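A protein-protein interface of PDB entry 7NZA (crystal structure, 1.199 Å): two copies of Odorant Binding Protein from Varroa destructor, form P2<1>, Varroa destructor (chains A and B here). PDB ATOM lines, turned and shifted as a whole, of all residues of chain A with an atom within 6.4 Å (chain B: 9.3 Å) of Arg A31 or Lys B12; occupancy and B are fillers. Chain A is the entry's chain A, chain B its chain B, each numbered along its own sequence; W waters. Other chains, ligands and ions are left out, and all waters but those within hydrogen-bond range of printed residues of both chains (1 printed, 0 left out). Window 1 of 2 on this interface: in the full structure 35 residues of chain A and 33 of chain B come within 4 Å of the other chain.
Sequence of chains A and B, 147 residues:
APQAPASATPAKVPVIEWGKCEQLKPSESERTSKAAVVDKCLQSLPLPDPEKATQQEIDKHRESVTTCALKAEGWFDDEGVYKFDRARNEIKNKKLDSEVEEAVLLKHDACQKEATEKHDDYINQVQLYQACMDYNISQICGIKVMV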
ATOM      1  N   VAL A  13       5.327 -26.434  -3.547  1.00  0.00           N
ATOM      2  CA  VAL A  13       4.255 -25.605  -4.136  1.00  0.00           C
ATOM      3  C   VAL A  13       2.925 -26.080  -3.559  1.00  0.00           C
ATOM      4  O   VAL A  13       2.760 -27.242  -3.212  1.00  0.00           O
ATOM      5  CB  VAL A  13       4.260 -25.674  -5.683  1.00  0.00           C
ATOM      6  CG1 VAL A  13       5.586 -25.174  -6.237  1.00  0.00           C
ATOM      7  CG2 VAL A  13       3.951 -27.033  -6.213  1.00  0.00           C
ATOM      8  N   PRO A  14       1.908 -25.200  -3.630  1.00  0.00           N
ATOM      9  CA  PRO A  14       0.568 -25.630  -3.282  1.00  0.00           C
ATOM     10  C   PRO A  14       0.039 -26.680  -4.242  1.00  0.00           C
ATOM     11  O   PRO A  14       0.333 -26.688  -5.406  1.00  0.00           O
ATOM     12  CB  PRO A  14      -0.291 -24.362  -3.353  1.00  0.00           C
ATOM     13  CG  PRO A  14       0.708 -23.200  -3.342  1.00  0.00           C
ATOM     14  CD  PRO A  14       1.977 -23.758  -3.934  1.00  0.00           C
ATOM     15  N   TRP A  18      -8.980 -26.451  -8.123  1.00  0.00           N
ATOM     16  CA  TRP A  18      -9.679 -25.173  -8.064  1.00  0.00           C
ATOM     17  C   TRP A  18     -11.179 -25.312  -8.306  1.00  0.00           C
ATOM     18  O   TRP A  18     -11.853 -24.297  -8.210  1.00  0.00           O
ATOM     19  CB  TRP A  18      -9.003 -24.211  -9.038  1.00  0.00           C
ATOM     20  CG  TRP A  18      -7.637 -23.829  -8.539  1.00  0.00           C
ATOM     21  CD1 TRP A  18      -6.455 -24.416  -8.871  1.00  0.00           C
ATOM     22  CD2 TRP A  18      -7.350 -22.849  -7.518  1.00  0.00           C
ATOM     23  NE1 TRP A  18      -5.448 -23.855  -8.125  1.00  0.00           N
ATOM     24  CE2 TRP A  18      -5.957 -22.920  -7.285  1.00  0.00           C
ATOM     25  CE3 TRP A  18      -8.112 -21.946  -6.794  1.00  0.00           C
ATOM     26  CZ2 TRP A  18      -5.338 -22.060  -6.366  1.00  0.00           C
ATOM     27  CZ3 TRP A  18      -7.490 -21.128  -5.906  1.00  0.00           C
ATOM     28  CH2 TRP A  18      -6.116 -21.192  -5.687  1.00  0.00           C
ATOM     29  N   LYS A  25      -6.729 -18.998  -8.981  1.00  0.00           N
ATOM     30  CA  LYS A  25      -5.334 -19.493  -8.889  1.00  0.00           C
ATOM     31  C   LYS A  25      -4.408 -18.297  -9.064  1.00  0.00           C
ATOM     32  O   LYS A  25      -4.536 -17.588 -10.059  1.00  0.00           O
ATOM     33  CB  LYS A  25      -5.142 -20.547  -9.956  1.00  0.00           C
ATOM     34  CG  LYS A  25      -3.735 -21.142 -10.026  1.00  0.00           C
ATOM     35  CD  LYS A  25      -3.734 -21.961 -11.304  1.00  0.00           C
ATOM     36  CE  LYS A  25      -2.645 -22.964 -11.499  1.00  0.00           C
ATOM     37  NZ  LYS A  25      -3.024 -23.902 -12.608  1.00  0.00           N
ATOM     38  N   PRO A  26      -3.442 -18.100  -8.152  1.00  0.00           N
ATOM     39  CA  PRO A  26      -2.495 -17.003  -8.337  1.00  0.00           C
ATOM     40  C   PRO A  26      -1.649 -17.214  -9.612  1.00  0.00           C
ATOM     41  O   PRO A  26      -1.240 -18.319  -9.914  1.00  0.00           O
ATOM     42  CB  PRO A  26      -1.622 -17.039  -7.075  1.00  0.00           C
ATOM     43  CG  PRO A  26      -2.412 -17.832  -6.036  1.00  0.00           C
ATOM     44  CD  PRO A  26      -3.229 -18.795  -6.873  1.00  0.00           C
ATOM     45  N   SER A  27      -1.426 -16.130 -10.295  1.00  0.00           N
ATOM     46  CA  SER A  27      -0.460 -16.192 -11.415  1.00  0.00           C
ATOM     47  C   SER A  27       0.980 -16.349 -10.884  1.00  0.00           C
ATOM     48  O   SER A  27       1.267 -15.993  -9.725  1.00  0.00           O
ATOM     49  CB  SER A  27      -0.585 -14.957 -12.281  1.00  0.00           C
ATOM     50  OG  SER A  27      -0.159 -13.824 -11.539  1.00  0.00           O
ATOM     51  N   GLU A  28       1.896 -16.805 -11.727  1.00  0.00           N
ATOM     52  CA  GLU A  28       3.359 -16.808 -11.421  1.00  0.00           C
ATOM     53  C   GLU A  28       3.729 -15.425 -10.906  1.00  0.00           C
ATOM     54  O   GLU A  28       4.492 -15.274  -9.950  1.00  0.00           O
ATOM     55  CB  GLU A  28       4.209 -17.186 -12.645  1.00  0.00           C
ATOM     56  CG  GLU A  28       5.721 -16.892 -12.562  1.00  0.00           C
ATOM     57  CD  GLU A  28       6.537 -17.112 -13.844  1.00  0.00           C
ATOM     58  OE1 GLU A  28       6.288 -16.364 -14.868  1.00  0.00           O
ATOM     59  OE2 GLU A  28       7.444 -17.984 -13.879  1.00  0.00           O
ATOM     60  N   SER A  29       3.231 -14.392 -11.575  1.00  0.00           N
ATOM     61  CA  SER A  29       3.593 -13.009 -11.235  1.00  0.00           C
ATOM     62  C   SER A  29       3.130 -12.647  -9.810  1.00  0.00           C
ATOM     63  O   SER A  29       3.887 -12.055  -9.018  1.00  0.00           O
ATOM     64  CB  SER A  29       3.119 -12.108 -12.329  1.00  0.00           C
ATOM     65  OG  SER A  29       3.417 -10.759 -11.998  1.00  0.00           O
ATOM     66  N   GLU A  30       1.930 -13.018  -9.477  1.00  0.00           N
ATOM     67  CA  GLU A  30       1.315 -12.721  -8.144  1.00  0.00           C
ATOM     68  C   GLU A  30       2.110 -13.452  -7.060  1.00  0.00           C
ATOM     69  O   GLU A  30       2.343 -12.924  -5.960  1.00  0.00           O
ATOM     70  CB  GLU A  30      -0.153 -13.185  -8.119  1.00  0.00           C
ATOM     71  CG  GLU A  30      -1.009 -12.137  -8.800  1.00  0.00           C
ATOM     72  CD  GLU A  30      -2.429 -12.518  -9.205  1.00  0.00           C
ATOM     73  OE1 GLU A  30      -2.792 -13.702  -9.054  1.00  0.00           O
ATOM     74  OE2 GLU A  30      -3.162 -11.596  -9.675  1.00  0.00           O
ATOM     75  N   ARG A  31       2.476 -14.673  -7.368  1.00  0.00           N
ATOM     76  CA  ARG A  31       3.277 -15.477  -6.463  1.00  0.00           C
ATOM     77  C   ARG A  31       4.648 -14.855  -6.223  1.00  0.00           C
ATOM     78  O   ARG A  31       5.073 -14.753  -5.083  1.00  0.00           O
ATOM     79  CB  ARG A  31       3.459 -16.864  -7.023  1.00  0.00           C
ATOM     80  CG  ARG A  31       4.138 -17.804  -6.089  1.00  0.00           C
ATOM     81  CD  ARG A  31       3.849 -19.205  -6.562  1.00  0.00           C
ATOM     82  NE  ARG A  31       2.418 -19.435  -6.489  1.00  0.00           N
ATOM     83  CZ  ARG A  31       1.687 -19.601  -5.376  1.00  0.00           C
ATOM     84  NH1 ARG A  31       2.198 -19.656  -4.163  1.00  0.00           N
ATOM     85  NH2 ARG A  31       0.400 -19.748  -5.538  1.00  0.00           N
ATOM     86  N   THR A  32       5.314 -14.455  -7.275  1.00  0.00           N
ATOM     87  CA  THR A  32       6.655 -13.840  -7.169  1.00  0.00           C
ATOM     88  C   THR A  32       6.543 -12.541  -6.355  1.00  0.00           C
ATOM     89  O   THR A  32       7.399 -12.269  -5.489  1.00  0.00           O
ATOM     90  CB  THR A  32       7.258 -13.613  -8.569  1.00  0.00           C
ATOM     91  OG1 THR A  32       7.468 -14.937  -9.097  1.00  0.00           O
ATOM     92  CG2 THR A  32       8.527 -12.768  -8.532  1.00  0.00           C
ATOM     93  N   SER A  33       5.514 -11.766  -6.623  1.00  0.00           N
ATOM     94  CA  SER A  33       5.208 -10.533  -5.869  1.00  0.00           C
ATOM     95  C   SER A  33       5.112 -10.797  -4.346  1.00  0.00           C
ATOM     96  O   SER A  33       5.694 -10.089  -3.548  1.00  0.00           O
ATOM     97  CB  SER A  33       3.958  -9.919  -6.382  1.00  0.00           C
ATOM     98  OG  SER A  33       3.674  -8.799  -5.584  1.00  0.00           O
ATOM     99  N   LYS A  34       4.276 -11.736  -3.987  1.00  0.00           N
ATOM    100  CA  LYS A  34       4.030 -12.052  -2.575  1.00  0.00           C
ATOM    101  C   LYS A  34       5.319 -12.534  -1.911  1.00  0.00           C
ATOM    102  O   LYS A  34       5.611 -12.197  -0.790  1.00  0.00           O
ATOM    103  CB  LYS A  34       2.958 -13.136  -2.477  1.00  0.00           C
ATOM    104  CG  LYS A  34       2.692 -13.543  -1.042  1.00  0.00           C
ATOM    105  CD  LYS A  34       2.200 -12.444  -0.141  1.00  0.00           C
ATOM    106  CE  LYS A  34       1.698 -12.879   1.193  1.00  0.00           C
ATOM    107  NZ  LYS A  34       0.366 -13.495   1.047  1.00  0.00           N
ATOM    108  N   ALA A  35       6.106 -13.358  -2.618  1.00  0.00           N
ATOM    109  CA  ALA A  35       7.372 -13.864  -2.069  1.00  0.00           C
ATOM    110  C   ALA A  35       8.272 -12.657  -1.778  1.00  0.00           C
ATOM    111  O   ALA A  35       9.000 -12.694  -0.748  1.00  0.00           O
ATOM    112  CB  ALA A  35       7.982 -14.805  -3.088  1.00  0.00           C
ATOM    113  N   ALA A  36       8.279 -11.666  -2.659  1.00  0.00           N
ATOM    114  CA  ALA A  36       9.177 -10.526  -2.438  1.00  0.00           C
ATOM    115  C   ALA A  36       8.770  -9.807  -1.164  1.00  0.00           C
ATOM    116  O   ALA A  36       9.607  -9.395  -0.356  1.00  0.00           O
ATOM    117  CB  ALA A  36       9.197  -9.603  -3.602  1.00  0.00           C
ATOM    118  N   ASP A 134     -11.611 -18.031   3.333  1.00  0.00           N
ATOM    119  CA  ASP A 134     -10.905 -19.265   2.850  1.00  0.00           C
ATOM    120  C   ASP A 134     -11.886 -20.416   2.881  1.00  0.00           C
ATOM    121  O   ASP A 134     -12.031 -21.147   1.883  1.00  0.00           O
ATOM    122  CB  ASP A 134      -9.668 -19.503   3.678  1.00  0.00           C
ATOM    123  CG  ASP A 134      -8.732 -20.554   3.140  1.00  0.00           C
ATOM    124  OD1 ASP A 134      -7.736 -20.207   2.554  1.00  0.00           O
ATOM    125  OD2 ASP A 134      -9.128 -21.696   3.230  1.00  0.00           O
ATOM    126  N   VAL A 145      -7.629 -28.644  -1.114  1.00  0.00           N
ATOM    127  CA  VAL A 145      -6.215 -28.265  -0.878  1.00  0.00           C
ATOM    128  C   VAL A 145      -5.551 -29.424  -0.146  1.00  0.00           C
ATOM    129  O   VAL A 145      -6.035 -29.838   0.857  1.00  0.00           O
ATOM    130  CB  VAL A 145      -6.118 -26.968  -0.043  1.00  0.00           C
ATOM    131  CG1 VAL A 145      -4.679 -26.551   0.229  1.00  0.00           C
ATOM    132  CG2 VAL A 145      -6.897 -25.842  -0.683  1.00  0.00           C
ATOM    133  N   SER B   7      -6.483  -9.142   1.339  1.00  0.00           N
ATOM    134  CA  SER B   7      -7.101  -9.932   0.280  1.00  0.00           C
ATOM    135  C   SER B   7      -7.908 -11.065   0.862  1.00  0.00           C
ATOM    136  O   SER B   7      -7.467 -11.706   1.840  1.00  0.00           O
ATOM    137  CB  SER B   7      -6.036 -10.515  -0.636  1.00  0.00           C
ATOM    138  OG  SER B   7      -6.576 -11.294  -1.674  1.00  0.00           O
ATOM    139  N   ALA B   8      -9.015 -11.411   0.195  1.00  0.00           N
ATOM    140  CA  ALA B   8      -9.750 -12.629   0.555  1.00  0.00           C
ATOM    141  C   ALA B   8      -9.025 -13.866   0.046  1.00  0.00           C
ATOM    142  O   ALA B   8      -9.384 -14.963   0.446  1.00  0.00           O
ATOM    143  CB  ALA B   8     -11.150 -12.531  -0.025  1.00  0.00           C
ATOM    144  N   THR B   9      -8.119 -13.753  -0.914  1.00  0.00           N
ATOM    145  CA  THR B   9      -7.461 -14.885  -1.566  1.00  0.00           C
ATOM    146  C   THR B   9      -5.933 -14.665  -1.657  1.00  0.00           C
ATOM    147  O   THR B   9      -5.354 -14.730  -2.757  1.00  0.00           O
ATOM    148  CB  THR B   9      -8.073 -15.160  -2.933  1.00  0.00           C
ATOM    149  OG1 THR B   9      -7.913 -14.045  -3.807  1.00  0.00           O
ATOM    150  CG2 THR B   9      -9.554 -15.467  -2.891  1.00  0.00           C
ATOM    151  N   PRO B  10      -5.271 -14.405  -0.540  1.00  0.00           N
ATOM    152  CA  PRO B  10      -3.807 -14.199  -0.612  1.00  0.00           C
ATOM    153  C   PRO B  10      -3.037 -15.414  -1.131  1.00  0.00           C
ATOM    154  O   PRO B  10      -3.356 -16.554  -0.806  1.00  0.00           O
ATOM    155  CB  PRO B  10      -3.484 -13.933   0.848  1.00  0.00           C
ATOM    156  CG  PRO B  10      -4.493 -14.707   1.643  1.00  0.00           C
ATOM    157  CD  PRO B  10      -5.765 -14.502   0.830  1.00  0.00           C
ATOM    158  N   ALA B  11      -2.000 -15.153  -1.936  1.00  0.00           N
ATOM    159  CA  ALA B  11      -1.071 -16.208  -2.336  1.00  0.00           C
ATOM    160  C   ALA B  11      -0.346 -16.712  -1.122  1.00  0.00           C
ATOM    161  O   ALA B  11       0.039 -15.903  -0.237  1.00  0.00           O
ATOM    162  CB  ALA B  11      -0.119 -15.699  -3.381  1.00  0.00           C
ATOM    163  N   LYS B  12      -0.129 -18.017  -1.070  1.00  0.00           N
ATOM    164  CA  LYS B  12       0.645 -18.641   0.018  1.00  0.00           C
ATOM    165  C   LYS B  12       2.014 -19.060  -0.506  1.00  0.00           C
ATOM    166  O   LYS B  12       2.105 -19.794  -1.481  1.00  0.00           O
ATOM    167  CB  LYS B  12      -0.214 -19.737   0.643  1.00  0.00           C
ATOM    168  CG  LYS B  12      -1.620 -19.303   1.100  1.00  0.00           C
ATOM    169  CD  LYS B  12      -2.604 -20.381   1.658  1.00  0.00           C
ATOM    170  CE  LYS B  12      -4.010 -19.876   1.887  1.00  0.00           C
ATOM    171  NZ  LYS B  12      -4.904 -20.929   2.439  1.00  0.00           N
ATOM    172  N   VAL B  13       3.042 -18.578   0.155  1.00  0.00           N
ATOM    173  CA  VAL B  13       4.440 -18.742  -0.274  1.00  0.00           C
ATOM    174  C   VAL B  13       5.230 -19.303   0.891  1.00  0.00           C
ATOM    175  O   VAL B  13       4.909 -19.101   2.048  1.00  0.00           O
ATOM    176  CB  VAL B  13       5.082 -17.427  -0.783  1.00  0.00           C
ATOM    177  CG1 VAL B  13       4.270 -16.852  -1.957  1.00  0.00           C
ATOM    178  CG2 VAL B  13       5.236 -16.360   0.287  1.00  0.00           C
ATOM    179  N   PRO B  14       6.355 -20.010   0.618  1.00  0.00           N
ATOM    180  CA  PRO B  14       7.265 -20.418   1.678  1.00  0.00           C
ATOM    181  C   PRO B  14       7.819 -19.204   2.409  1.00  0.00           C
ATOM    182  O   PRO B  14       8.063 -18.179   1.892  1.00  0.00           O
ATOM    183  CB  PRO B  14       8.340 -21.205   0.971  1.00  0.00           C
ATOM    184  CG  PRO B  14       7.735 -21.626  -0.379  1.00  0.00           C
ATOM    185  CD  PRO B  14       6.791 -20.482  -0.718  1.00  0.00           C
ATOM    186  N   VAL B  15       7.968 -19.412   3.701  1.00  0.00           N
ATOM    187  CA  VAL B  15       8.536 -18.417   4.639  1.00  0.00           C
ATOM    188  C   VAL B  15       9.784 -19.051   5.224  1.00  0.00           C
ATOM    189  O   VAL B  15       9.674 -19.880   6.145  1.00  0.00           O
ATOM    190  CB  VAL B  15       7.489 -18.039   5.674  1.00  0.00           C
ATOM    191  CG1 VAL B  15       8.075 -17.001   6.554  1.00  0.00           C
ATOM    192  CG2 VAL B  15       6.193 -17.551   5.065  1.00  0.00           C
ATOM    193  N   SER B  27      14.670 -20.819  -7.744  1.00  0.00           N
ATOM    194  CA  SER B  27      14.387 -19.700  -8.654  1.00  0.00           C
ATOM    195  C   SER B  27      12.897 -19.634  -8.991  1.00  0.00           C
ATOM    196  O   SER B  27      12.172 -20.599  -8.883  1.00  0.00           O
ATOM    197  CB  SER B  27      15.193 -19.784  -9.887  1.00  0.00           C
ATOM    198  OG  SER B  27      14.762 -20.881 -10.674  1.00  0.00           O
ATOM    199  N   GLU B  28      12.461 -18.500  -9.541  1.00  0.00           N
ATOM    200  CA  GLU B  28      11.089 -18.359 -10.049  1.00  0.00           C
ATOM    201  C   GLU B  28      10.876 -19.448 -11.107  1.00  0.00           C
ATOM    202  O   GLU B  28       9.809 -20.078 -11.126  1.00  0.00           O
ATOM    203  CB  GLU B  28      10.834 -16.976 -10.664  1.00  0.00           C
ATOM    204  CG  GLU B  28       9.437 -16.774 -11.278  1.00  0.00           C
ATOM    205  CD  GLU B  28       9.309 -15.408 -11.920  1.00  0.00           C
ATOM    206  OE1 GLU B  28      10.109 -15.124 -12.903  1.00  0.00           O
ATOM    207  OE2 GLU B  28       8.427 -14.628 -11.501  1.00  0.00           O
ATOM    208  N   GLU B  30      12.236 -22.441 -11.451  1.00  0.00           N
ATOM    209  CA  GLU B  30      12.143 -23.757 -10.801  1.00  0.00           C
ATOM    210  C   GLU B  30      10.778 -23.878 -10.126  1.00  0.00           C
ATOM    211  O   GLU B  30      10.144 -24.937 -10.179  1.00  0.00           O
ATOM    212  CB  GLU B  30      13.272 -23.899  -9.767  1.00  0.00           C
ATOM    213  CG  GLU B  30      14.590 -24.196 -10.436  1.00  0.00           C
ATOM    214  CD  GLU B  30      15.858 -24.039  -9.586  1.00  0.00           C
ATOM    215  OE1 GLU B  30      16.963 -24.276 -10.126  1.00  0.00           O
ATOM    216  OE2 GLU B  30      15.775 -23.436  -8.540  1.00  0.00           O
ATOM    217  N   ARG B  31      10.353 -22.814  -9.480  1.00  0.00           N
ATOM    218  CA  ARG B  31       9.025 -22.807  -8.813  1.00  0.00           C
ATOM    219  C   ARG B  31       7.890 -22.985  -9.816  1.00  0.00           C
ATOM    220  O   ARG B  31       6.974 -23.768  -9.590  1.00  0.00           O
ATOM    221  CB  ARG B  31       8.742 -21.457  -8.153  1.00  0.00           C
ATOM    222  CG  ARG B  31       7.838 -21.539  -6.944  1.00  0.00           C
ATOM    223  CD  ARG B  31       7.538 -20.068  -6.651  1.00  0.00           C
ATOM    224  NE  ARG B  31       6.778 -19.486  -7.753  1.00  0.00           N
ATOM    225  CZ  ARG B  31       6.887 -18.242  -8.213  1.00  0.00           C
ATOM    226  NH1 ARG B  31       7.721 -17.363  -7.684  1.00  0.00           N
ATOM    227  NH2 ARG B  31       6.146 -17.897  -9.218  1.00  0.00           N
ATOM    228  N   THR B  32       7.961 -22.268 -10.921  1.00  0.00           N
ATOM    229  CA  THR B  32       6.931 -22.335 -11.951  1.00  0.00           C
ATOM    230  C   THR B  32       6.938 -23.718 -12.596  1.00  0.00           C
ATOM    231  O   THR B  32       5.836 -24.270 -12.817  1.00  0.00           O
ATOM    232  CB  THR B  32       7.149 -21.245 -12.989  1.00  0.00           C
ATOM    233  OG1 THR B  32       6.971 -20.005 -12.289  1.00  0.00           O
ATOM    234  CG2 THR B  32       6.161 -21.343 -14.131  1.00  0.00           C
ATOM    235  N   SER B  33       8.103 -24.329 -12.838  1.00  0.00           N
ATOM    236  CA  SER B  33       8.121 -25.682 -13.394  1.00  0.00           C
ATOM    237  C   SER B  33       7.483 -26.639 -12.408  1.00  0.00           C
ATOM    238  O   SER B  33       6.782 -27.545 -12.807  1.00  0.00           O
ATOM    239  CB  SER B  33       9.499 -26.095 -13.650  1.00  0.00           C
ATOM    240  OG  SER B  33      10.065 -25.403 -14.755  1.00  0.00           O
ATOM    241  N   LYS B  34       7.824 -26.545 -11.112  1.00  0.00           N
ATOM    242  CA  LYS B  34       7.247 -27.487 -10.143  1.00  0.00           C
ATOM    243  C   LYS B  34       5.723 -27.358 -10.091  1.00  0.00           C
ATOM    244  O   LYS B  34       5.016 -28.327 -10.036  1.00  0.00           O
ATOM    245  CB  LYS B  34       7.881 -27.237  -8.766  1.00  0.00           C
ATOM    246  CG  LYS B  34       7.392 -28.215  -7.706  1.00  0.00           C
ATOM    247  CD  LYS B  34       7.583 -29.704  -8.048  1.00  0.00           C
ATOM    248  CE  LYS B  34       7.295 -30.639  -6.899  1.00  0.00           C
ATOM    249  NZ  LYS B  34       8.365 -30.593  -5.874  1.00  0.00           N
ATOM    250  N   ALA B  35       5.199 -26.141 -10.134  1.00  0.00           N
ATOM    251  CA  ALA B  35       3.718 -25.937 -10.201  1.00  0.00           C
ATOM    252  C   ALA B  35       3.165 -26.567 -11.453  1.00  0.00           C
ATOM    253  O   ALA B  35       2.094 -27.177 -11.374  1.00  0.00           O
ATOM    254  CB  ALA B  35       3.386 -24.475 -10.126  1.00  0.00           C
ATOM    255  N   ASP B  39       0.440 -29.549 -11.315  1.00  0.00           N
ATOM    256  CA  ASP B  39      -0.909 -29.327 -11.862  1.00  0.00           C
ATOM    257  C   ASP B  39      -1.144 -30.399 -12.880  1.00  0.00           C
ATOM    258  O   ASP B  39      -2.293 -30.928 -12.956  1.00  0.00           O
ATOM    259  CB  ASP B  39      -1.037 -27.921 -12.405  1.00  0.00           C
ATOM    260  CG  ASP B  39      -1.103 -26.888 -11.294  1.00  0.00           C
ATOM    261  OD1 ASP B  39      -1.374 -27.262 -10.111  1.00  0.00           O
ATOM    262  OD2 ASP B  39      -0.863 -25.698 -11.617  1.00  0.00           O
HETATM  263  O   HOH W   1      -1.631 -26.869  -7.384  1.00  0.00           O
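The side-chain carboxylate of Asp B39 is in salt-bridge range of the side-chain amino group of Lys A25.
The backbone carbonyl oxygen (O) of Glu A28 is in hydrogen-bond range of the guanidinium group (NH2) of Arg B31, 3.2 Å away.
OG1 of Thr B32 is in hydrogen-bond range of OE2 of Glu A28 (2.6 Å).
The guanidinium group (NH1) of Arg A31 is in hydrogen-bond range of the backbone carbonyl oxygen (O) of Lys B12 (2.7 Å).
OG1 of Thr A32 lies within hydrogen-bond range of OE2 of Glu B28.
The side-chain hydroxyl (OG1) of Thr A32 sits at hydrogen-bond distance from the guanidinium group (NH1) of Arg B31 (2.8 Å).
The side-chain amino group (NZ) of Lys A34 is in hydrogen-bond range of the backbone carbonyl oxygen (O) of Ala B11, 2.7 Å away.
The side-chain carboxylate of Asp A134 is in salt-bridge range of the side-chain amino group of Lys B12 (2.9 Å).
The side-chain hydroxyl (OG1) of Thr A32 sits at hydrogen-bond distance from the backbone carbonyl oxygen (O) of Glu A28 (3.1 Å).
The backbone carbonyl oxygen (O) of Glu B28 lies within hydrogen-bond range of the side-chain hydroxyl (OG1) of Thr B32 (3.1 Å).
Among the printed residues, pairs that only touch across the chains: Arg A31 with Arg B31 (3.2 Å), Glu A28 with Glu B28 (3.5 Å), Lys A34 with Val B13 (3.8 Å), Val A13 with Lys B34 (3.8 Å), Arg A31 with Val B13 (3.8 Å), Lys A34 with Pro B10 (3.9 Å) and Val A13 with Arg B31 (3.9 Å).
Printed residues of chain B within 4 Å of Val A13: Arg B31 and Lys B34.
Trp A18 touches none of the printed residues of chain B.
No residue of chain B comes within 4 Å of Pro A26.
Of the printed residues of chain B, Arg A31 touches Lys B12 (2.7 Å), Val B13 (3.8 Å) and Arg B31 (3.2 Å).
Of the printed residues of chain B, Lys A34 touches Pro B10, Ala B11 and Val B13.
Printed residues of chain B within 4 Å of Asp A134: Lys B12.
Of the printed residues of chain A, Pro B10 touches Lys A34 (3.9 Å).
Lys B12 touches just these residues of chain A: Arg A31 (2.7 Å) and Asp A134 (2.9 Å).
The nearest residue of chain A that does not touch Lys B12 is Pro A14 (4.1 Å).
Hydrophobic or aromatic side chains of chain B within 4 Å of the printed part of chain A: Pro B10 and Val B13.
Hydrophobic or aromatic side chains of chain A that line the printed part of chain B: Val A13.
Along chain A the printed residues that touch a printed residue of chain B span positions 13 to 134.
Among the printed residues, 15 pairs touch across the chains.
Among the printed residues, Asp or Glu carboxylates within 4 Å of a Lys or Arg side-chain nitrogen of the other chain: Lys A25 with Asp B39 and Asp A134 with Lys B12.
Val A13 touches Lys B34, and with the chains exchanged Lys A34 touches Val B13.
Glu A28 touches Arg B31, but with the chains exchanged Arg A31 does not touch Glu B28 (6.5 Å).
Glu A28 touches Thr B32, and with the chains exchanged Thr A32 touches Glu B28.
Arg A31 touches its own counterpart, Arg B31.
Positions printed for both chains: 13, 14, 27, 28, 30, 31, 32, 33, 34 and 35.
Of the 15 pairs that touch across the chains among the printed residues, 8 have their exchanged pair printed and touching as well.
Water W1 lies within hydrogen-bond range of the side-chain carboxylate (OD1) of Asp B39 (2.8 Å) and the backbone carbonyl oxygen (O) of Pro A14 (2.8 Å).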
